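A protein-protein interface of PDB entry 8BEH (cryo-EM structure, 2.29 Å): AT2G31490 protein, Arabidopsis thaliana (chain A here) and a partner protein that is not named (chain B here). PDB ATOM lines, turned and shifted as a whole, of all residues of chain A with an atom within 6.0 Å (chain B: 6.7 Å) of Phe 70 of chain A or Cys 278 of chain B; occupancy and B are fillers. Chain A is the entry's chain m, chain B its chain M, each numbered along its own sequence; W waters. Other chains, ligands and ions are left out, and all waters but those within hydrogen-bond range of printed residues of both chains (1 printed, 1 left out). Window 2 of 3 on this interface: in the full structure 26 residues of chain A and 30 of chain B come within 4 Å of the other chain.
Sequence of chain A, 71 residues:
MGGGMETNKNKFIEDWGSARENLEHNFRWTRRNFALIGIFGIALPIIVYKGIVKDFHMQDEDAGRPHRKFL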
ATOM      1  N   TYR A  49     -20.025  32.561 -29.937  1.00  0.00           N
ATOM      2  CA  TYR A  49     -20.220  31.135 -29.702  1.00  0.00           C
ATOM      3  C   TYR A  49     -20.123  30.801 -28.218  1.00  0.00           C
ATOM      4  O   TYR A  49     -20.946  30.045 -27.689  1.00  0.00           O
ATOM      5  CB  TYR A  49     -19.197  30.326 -30.503  1.00  0.00           C
ATOM      6  CG  TYR A  49     -19.286  28.837 -30.273  1.00  0.00           C
ATOM      7  CD1 TYR A  49     -18.524  28.213 -29.292  1.00  0.00           C
ATOM      8  CD2 TYR A  49     -20.135  28.050 -31.040  1.00  0.00           C
ATOM      9  CE1 TYR A  49     -18.611  26.851 -29.079  1.00  0.00           C
ATOM     10  CE2 TYR A  49     -20.226  26.691 -30.836  1.00  0.00           C
ATOM     11  CZ  TYR A  49     -19.461  26.097 -29.854  1.00  0.00           C
ATOM     12  OH  TYR A  49     -19.552  24.746 -29.653  1.00  0.00           O
ATOM     13  N   VAL A  53     -23.182  29.200 -25.810  1.00  0.00           N
ATOM     14  CA  VAL A  53     -22.932  27.930 -25.096  1.00  0.00           C
ATOM     15  C   VAL A  53     -23.157  28.130 -23.593  1.00  0.00           C
ATOM     16  O   VAL A  53     -23.800  27.332 -23.016  1.00  0.00           O
ATOM     17  CB  VAL A  53     -21.568  27.272 -25.456  1.00  0.00           C
ATOM     18  CG1 VAL A  53     -21.129  26.202 -24.472  1.00  0.00           C
ATOM     19  CG2 VAL A  53     -21.506  26.773 -26.890  1.00  0.00           C
ATOM     20  N   PHE A  56     -26.803  28.187 -22.705  1.00  0.00           N
ATOM     21  CA  PHE A  56     -27.302  26.819 -22.492  1.00  0.00           C
ATOM     22  C   PHE A  56     -26.806  26.216 -21.143  1.00  0.00           C
ATOM     23  O   PHE A  56     -27.575  25.485 -20.564  1.00  0.00           O
ATOM     24  CB  PHE A  56     -27.005  25.870 -23.663  1.00  0.00           C
ATOM     25  CG  PHE A  56     -27.723  26.108 -24.971  1.00  0.00           C
ATOM     26  CD1 PHE A  56     -29.097  25.948 -25.079  1.00  0.00           C
ATOM     27  CD2 PHE A  56     -27.016  26.410 -26.122  1.00  0.00           C
ATOM     28  CE1 PHE A  56     -29.745  26.113 -26.291  1.00  0.00           C
ATOM     29  CE2 PHE A  56     -27.662  26.585 -27.337  1.00  0.00           C
ATOM     30  CZ  PHE A  56     -29.026  26.428 -27.426  1.00  0.00           C
ATOM     31  N   HIS A  57     -25.560  26.436 -20.750  1.00  0.00           N
ATOM     32  CA  HIS A  57     -24.967  25.847 -19.511  1.00  0.00           C
ATOM     33  C   HIS A  57     -25.610  26.479 -18.293  1.00  0.00           C
ATOM     34  O   HIS A  57     -25.836  25.777 -17.338  1.00  0.00           O
ATOM     35  CB  HIS A  57     -23.428  26.011 -19.523  1.00  0.00           C
ATOM     36  CG  HIS A  57     -22.703  25.116 -20.465  1.00  0.00           C
ATOM     37  ND1 HIS A  57     -21.362  25.285 -20.764  1.00  0.00           N
ATOM     38  CD2 HIS A  57     -23.108  24.028 -21.144  1.00  0.00           C
ATOM     39  CE1 HIS A  57     -20.989  24.339 -21.588  1.00  0.00           C
ATOM     40  NE2 HIS A  57     -22.034  23.565 -21.840  1.00  0.00           N
ATOM     41  N   ASP A  60     -28.687  24.870 -18.036  1.00  0.00           N
ATOM     42  CA  ASP A  60     -28.471  23.515 -17.538  1.00  0.00           C
ATOM     43  C   ASP A  60     -28.351  23.500 -16.020  1.00  0.00           C
ATOM     44  O   ASP A  60     -28.991  22.689 -15.341  1.00  0.00           O
ATOM     45  CB  ASP A  60     -27.219  22.917 -18.174  1.00  0.00           C
ATOM     46  CG  ASP A  60     -27.503  22.259 -19.500  1.00  0.00           C
ATOM     47  OD1 ASP A  60     -28.685  21.967 -19.768  1.00  0.00           O
ATOM     48  OD2 ASP A  60     -26.550  22.038 -20.277  1.00  0.00           O
ATOM     49  N   ARG A  68     -24.444  20.501 -20.966  1.00  0.00           N
ATOM     50  CA  ARG A  68     -24.655  19.783 -22.213  1.00  0.00           C
ATOM     51  C   ARG A  68     -23.392  19.873 -23.058  1.00  0.00           C
ATOM     52  O   ARG A  68     -22.840  20.960 -23.246  1.00  0.00           O
ATOM     53  CB  ARG A  68     -25.841  20.385 -22.960  1.00  0.00           C
ATOM     54  CG  ARG A  68     -26.877  19.393 -23.437  1.00  0.00           C
ATOM     55  CD  ARG A  68     -28.042  20.132 -24.078  1.00  0.00           C
ATOM     56  NE  ARG A  68     -28.689  21.038 -23.133  1.00  0.00           N
ATOM     57  CZ  ARG A  68     -28.794  22.348 -23.310  1.00  0.00           C
ATOM     58  NH1 ARG A  68     -28.351  22.932 -24.410  1.00  0.00           N
ATOM     59  NH2 ARG A  68     -29.364  23.091 -22.365  1.00  0.00           N
ATOM     60  N   LYS A  69     -22.926  18.734 -23.557  1.00  0.00           N
ATOM     61  CA  LYS A  69     -21.771  18.747 -24.440  1.00  0.00           C
ATOM     62  C   LYS A  69     -22.175  19.232 -25.826  1.00  0.00           C
ATOM     63  O   LYS A  69     -23.308  19.036 -26.272  1.00  0.00           O
ATOM     64  CB  LYS A  69     -21.115  17.363 -24.514  1.00  0.00           C
ATOM     65  CG  LYS A  69     -20.446  16.842 -23.239  1.00  0.00           C
ATOM     66  CD  LYS A  69     -19.844  15.452 -23.398  1.00  0.00           C
ATOM     67  CE  LYS A  69     -19.172  14.994 -22.116  1.00  0.00           C
ATOM     68  NZ  LYS A  69     -18.600  13.626 -22.251  1.00  0.00           N
ATOM     69  N   PHE A  70     -21.239  19.894 -26.502  1.00  0.00           N
ATOM     70  CA  PHE A  70     -21.520  20.513 -27.787  1.00  0.00           C
ATOM     71  C   PHE A  70     -20.377  20.259 -28.760  1.00  0.00           C
ATOM     72  O   PHE A  70     -19.231  20.054 -28.355  1.00  0.00           O
ATOM     73  CB  PHE A  70     -21.766  22.014 -27.623  1.00  0.00           C
ATOM     74  CG  PHE A  70     -23.092  22.346 -26.993  1.00  0.00           C
ATOM     75  CD1 PHE A  70     -24.273  21.904 -27.564  1.00  0.00           C
ATOM     76  CD2 PHE A  70     -23.154  23.090 -25.825  1.00  0.00           C
ATOM     77  CE1 PHE A  70     -25.493  22.213 -26.994  1.00  0.00           C
ATOM     78  CE2 PHE A  70     -24.370  23.397 -25.245  1.00  0.00           C
ATOM     79  CZ  PHE A  70     -25.541  22.959 -25.829  1.00  0.00           C
ATOM     80  N   LEU A  71     -20.710  20.273 -30.050  1.00  0.00           N
ATOM     81  CA  LEU A  71     -19.755  20.042 -31.139  1.00  0.00           C
ATOM     82  C   LEU A  71     -19.156  18.642 -31.068  1.00  0.00           C
ATOM     83  O   LEU A  71     -19.858  17.669 -30.789  1.00  0.00           O
ATOM     84  CB  LEU A  71     -18.637  21.093 -31.117  1.00  0.00           C
ATOM     85  CG  LEU A  71     -18.888  22.388 -31.884  1.00  0.00           C
ATOM     86  CD1 LEU A  71     -17.671  23.297 -31.831  1.00  0.00           C
ATOM     87  CD2 LEU A  71     -19.255  22.086 -33.319  1.00  0.00           C
ATOM     88  N   PRO B 273     -30.641  13.467 -34.957  1.00  0.00           N
ATOM     89  CA  PRO B 273     -31.068  14.411 -33.909  1.00  0.00           C
ATOM     90  C   PRO B 273     -29.987  14.723 -32.885  1.00  0.00           C
ATOM     91  O   PRO B 273     -29.905  15.865 -32.418  1.00  0.00           O
ATOM     92  CB  PRO B 273     -32.276  13.706 -33.273  1.00  0.00           C
ATOM     93  CG  PRO B 273     -32.090  12.267 -33.586  1.00  0.00           C
ATOM     94  CD  PRO B 273     -31.393  12.200 -34.907  1.00  0.00           C
ATOM     95  N   GLU B 274     -29.135  13.752 -32.544  1.00  0.00           N
ATOM     96  CA  GLU B 274     -28.082  14.000 -31.563  1.00  0.00           C
ATOM     97  C   GLU B 274     -27.039  14.969 -32.108  1.00  0.00           C
ATOM     98  O   GLU B 274     -26.615  15.893 -31.405  1.00  0.00           O
ATOM     99  CB  GLU B 274     -27.415  12.688 -31.137  1.00  0.00           C
ATOM    100  CG  GLU B 274     -28.292  11.684 -30.382  1.00  0.00           C
ATOM    101  CD  GLU B 274     -29.623  11.399 -31.049  1.00  0.00           C
ATOM    102  OE1 GLU B 274     -29.637  10.694 -32.081  1.00  0.00           O
ATOM    103  OE2 GLU B 274     -30.656  11.887 -30.544  1.00  0.00           O
ATOM    104  N   ALA B 275     -26.611  14.770 -33.356  1.00  0.00           N
ATOM    105  CA  ALA B 275     -25.707  15.723 -33.987  1.00  0.00           C
ATOM    106  C   ALA B 275     -26.367  17.087 -34.133  1.00  0.00           C
ATOM    107  O   ALA B 275     -25.726  18.121 -33.914  1.00  0.00           O
ATOM    108  CB  ALA B 275     -25.251  15.198 -35.347  1.00  0.00           C
ATOM    109  N   THR B 276     -27.650  17.105 -34.503  1.00  0.00           N
ATOM    110  CA  THR B 276     -28.386  18.361 -34.596  1.00  0.00           C
ATOM    111  C   THR B 276     -28.332  19.117 -33.279  1.00  0.00           C
ATOM    112  O   THR B 276     -28.147  20.338 -33.259  1.00  0.00           O
ATOM    113  CB  THR B 276     -29.837  18.093 -35.008  1.00  0.00           C
ATOM    114  OG1 THR B 276     -29.871  17.515 -36.318  1.00  0.00           O
ATOM    115  CG2 THR B 276     -30.658  19.374 -34.992  1.00  0.00           C
ATOM    116  N   LEU B 277     -28.476  18.400 -32.166  1.00  0.00           N
ATOM    117  CA  LEU B 277     -28.352  19.017 -30.853  1.00  0.00           C
ATOM    118  C   LEU B 277     -26.930  19.518 -30.614  1.00  0.00           C
ATOM    119  O   LEU B 277     -26.727  20.644 -30.149  1.00  0.00           O
ATOM    120  CB  LEU B 277     -28.765  18.009 -29.781  1.00  0.00           C
ATOM    121  CG  LEU B 277     -29.332  18.522 -28.460  1.00  0.00           C
ATOM    122  CD1 LEU B 277     -30.021  17.383 -27.738  1.00  0.00           C
ATOM    123  CD2 LEU B 277     -28.264  19.149 -27.590  1.00  0.00           C
ATOM    124  N   CYS B 278     -25.932  18.695 -30.947  1.00  0.00           N
ATOM    125  CA  CYS B 278     -24.544  19.055 -30.673  1.00  0.00           C
ATOM    126  C   CYS B 278     -24.119  20.298 -31.448  1.00  0.00           C
ATOM    127  O   CYS B 278     -23.354  21.124 -30.938  1.00  0.00           O
ATOM    128  CB  CYS B 278     -23.622  17.879 -31.005  1.00  0.00           C
ATOM    129  SG  CYS B 278     -23.618  16.553 -29.781  1.00  0.00           S
ATOM    130  N   PHE B 279     -24.612  20.456 -32.673  1.00  0.00           N
ATOM    131  CA  PHE B 279     -24.201  21.553 -33.540  1.00  0.00           C
ATOM    132  C   PHE B 279     -25.071  22.799 -33.411  1.00  0.00           C
ATOM    133  O   PHE B 279     -24.809  23.784 -34.105  1.00  0.00           O
ATOM    134  CB  PHE B 279     -24.187  21.081 -34.997  1.00  0.00           C
ATOM    135  CG  PHE B 279     -22.992  20.248 -35.344  1.00  0.00           C
ATOM    136  CD1 PHE B 279     -21.744  20.829 -35.478  1.00  0.00           C
ATOM    137  CD2 PHE B 279     -23.108  18.879 -35.491  1.00  0.00           C
ATOM    138  CE1 PHE B 279     -20.638  20.062 -35.783  1.00  0.00           C
ATOM    139  CE2 PHE B 279     -22.009  18.107 -35.791  1.00  0.00           C
ATOM    140  CZ  PHE B 279     -20.770  18.698 -35.937  1.00  0.00           C
ATOM    141  N   THR B 280     -26.082  22.788 -32.544  1.00  0.00           N
ATOM    142  CA  THR B 280     -26.994  23.929 -32.460  1.00  0.00           C
ATOM    143  C   THR B 280     -26.293  25.236 -32.101  1.00  0.00           C
ATOM    144  O   THR B 280     -26.586  26.258 -32.745  1.00  0.00           O
ATOM    145  CB  THR B 280     -28.135  23.604 -31.488  1.00  0.00           C
ATOM    146  OG1 THR B 280     -28.976  22.604 -32.069  1.00  0.00           O
ATOM    147  CG2 THR B 280     -28.965  24.848 -31.182  1.00  0.00           C
ATOM    148  N   PRO B 281     -25.388  25.295 -31.115  1.00  0.00           N
ATOM    149  CA  PRO B 281     -24.665  26.560 -30.890  1.00  0.00           C
ATOM    150  C   PRO B 281     -23.878  27.027 -32.101  1.00  0.00           C
ATOM    151  O   PRO B 281     -23.811  28.231 -32.369  1.00  0.00           O
ATOM    152  CB  PRO B 281     -23.750  26.229 -29.702  1.00  0.00           C
ATOM    153  CG  PRO B 281     -24.418  25.106 -29.019  1.00  0.00           C
ATOM    154  CD  PRO B 281     -25.037  24.288 -30.097  1.00  0.00           C
ATOM    155  N   PHE B 282     -23.294  26.093 -32.853  1.00  0.00           N
ATOM    156  CA  PHE B 282     -22.535  26.447 -34.047  1.00  0.00           C
ATOM    157  C   PHE B 282     -23.434  27.090 -35.102  1.00  0.00           C
ATOM    158  O   PHE B 282     -23.098  28.139 -35.669  1.00  0.00           O
ATOM    159  CB  PHE B 282     -21.841  25.191 -34.582  1.00  0.00           C
ATOM    160  CG  PHE B 282     -21.141  25.382 -35.891  1.00  0.00           C
ATOM    161  CD1 PHE B 282     -19.992  26.147 -35.974  1.00  0.00           C
ATOM    162  CD2 PHE B 282     -21.618  24.769 -37.038  1.00  0.00           C
ATOM    163  CE1 PHE B 282     -19.340  26.311 -37.180  1.00  0.00           C
ATOM    164  CE2 PHE B 282     -20.971  24.930 -38.246  1.00  0.00           C
ATOM    165  CZ  PHE B 282     -19.829  25.703 -38.315  1.00  0.00           C
ATOM    166  N   ARG B 410     -35.479  28.794 -26.515  1.00  0.00           N
ATOM    167  CA  ARG B 410     -34.279  27.973 -26.398  1.00  0.00           C
ATOM    168  C   ARG B 410     -33.091  28.769 -25.867  1.00  0.00           C
ATOM    169  O   ARG B 410     -32.410  28.329 -24.939  1.00  0.00           O
ATOM    170  CB  ARG B 410     -33.917  27.353 -27.754  1.00  0.00           C
ATOM    171  CG  ARG B 410     -34.961  26.426 -28.323  1.00  0.00           C
ATOM    172  CD  ARG B 410     -34.919  25.050 -27.678  1.00  0.00           C
ATOM    173  NE  ARG B 410     -33.570  24.629 -27.320  1.00  0.00           N
ATOM    174  CZ  ARG B 410     -32.751  23.962 -28.120  1.00  0.00           C
ATOM    175  NH1 ARG B 410     -33.097  23.644 -29.357  1.00  0.00           N
ATOM    176  NH2 ARG B 410     -31.552  23.609 -27.671  1.00  0.00           N
HETATM  177  O   HOH W   1     -22.191  23.743 -31.456  1.00  0.00           O
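NH2 of Arg 68 of chain A is in hydrogen-bond range of O of Phe 56 of chain A (3.5 Å).
A ring nitrogen (NE2) of His 57 of chain A is in hydrogen-bond range of the backbone carbonyl oxygen (O) of Arg 68 of chain A, 3.1 Å away.
The side-chain carboxylate of Asp 60 of chain A is in salt-bridge range of the guanidinium group of Arg 68 of chain A.
The backbone carbonyl oxygen of Glu 274 of chain B lies within hydrogen-bond range of the side-chain sulfur of Cys 278 of chain B (3.5 Å).
Of the 11 printed residues of chain B, 6 touch a printed residue of chain A.
Hydrophobic or aromatic side chains of chain B within 4 Å of the printed part of chain A: Leu 277, Phe 279 and Pro 281.
Printed residues of chain A that touch a printed residue of chain B: Tyr 49, Val 53, Phe 56, Arg 68, Phe 70 and Leu 71.
Among the printed residues, 11 pairs touch across the chains.
Among the printed residues, no Asp or Glu carboxylate lies within 4 Å of a Lys or Arg side-chain nitrogen of the other chain.
Water W1 lies within hydrogen-bond range of the backbone carbonyl oxygen (O) of Cys 278 of chain B, the backbone NH (N) of Phe 282 of chain B and the side-chain hydroxyl (OH) of Tyr 49 of chain A.
Phe 70 of chain A touches just these residues of chain B: Leu 277, Cys 278 and Pro 281.
Of the printed residues of chain A, Phe 282 of chain B touches Tyr 49.
Printed residues of chain B within 4 Å of Phe 56 of chain A: Pro 281 (3.9 Å) and Arg 410 (3.4 Å).
Ala 275 of chain B touches none of the printed residues of chain A.
The nearest residue of chain B that does not touch Phe 70 of chain A is Phe 279 of chain B (5.3 Å).
The nearest printed residue of chain A that does not touch Phe 279 of chain B is Phe 70 of chain A (5.3 Å).
Among the printed residues, merely in contact across the chains: Tyr 49 of chain A with Pro 281 of chain B (3.7 Å), Tyr 49 of chain A with Phe 282 of chain B (3.7 Å), Val 53 of chain A with Pro 281 of chain B (3.6 Å), Phe 56 of chain A with Pro 281 of chain B (3.9 Å), Phe 56 of chain A with Arg 410 of chain B (3.4 Å), Arg 68 of chain A with Leu 277 of chain B (3.7 Å), Phe 70 of chain A with Leu 277 of chain B (3.7 Å), Phe 70 of chain A with Cys 278 of chain B (3.6 Å), Phe 70 of chain A with Pro 281 of chain B (3.5 Å) and Leu 71 of chain A with Phe 279 of chain B (3.5 Å).
The backbone NH (N) of Leu 71 of chain A lies within hydrogen-bond range of the backbone carbonyl oxygen (O) of Cys 278 of chain B (2.9 Å).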
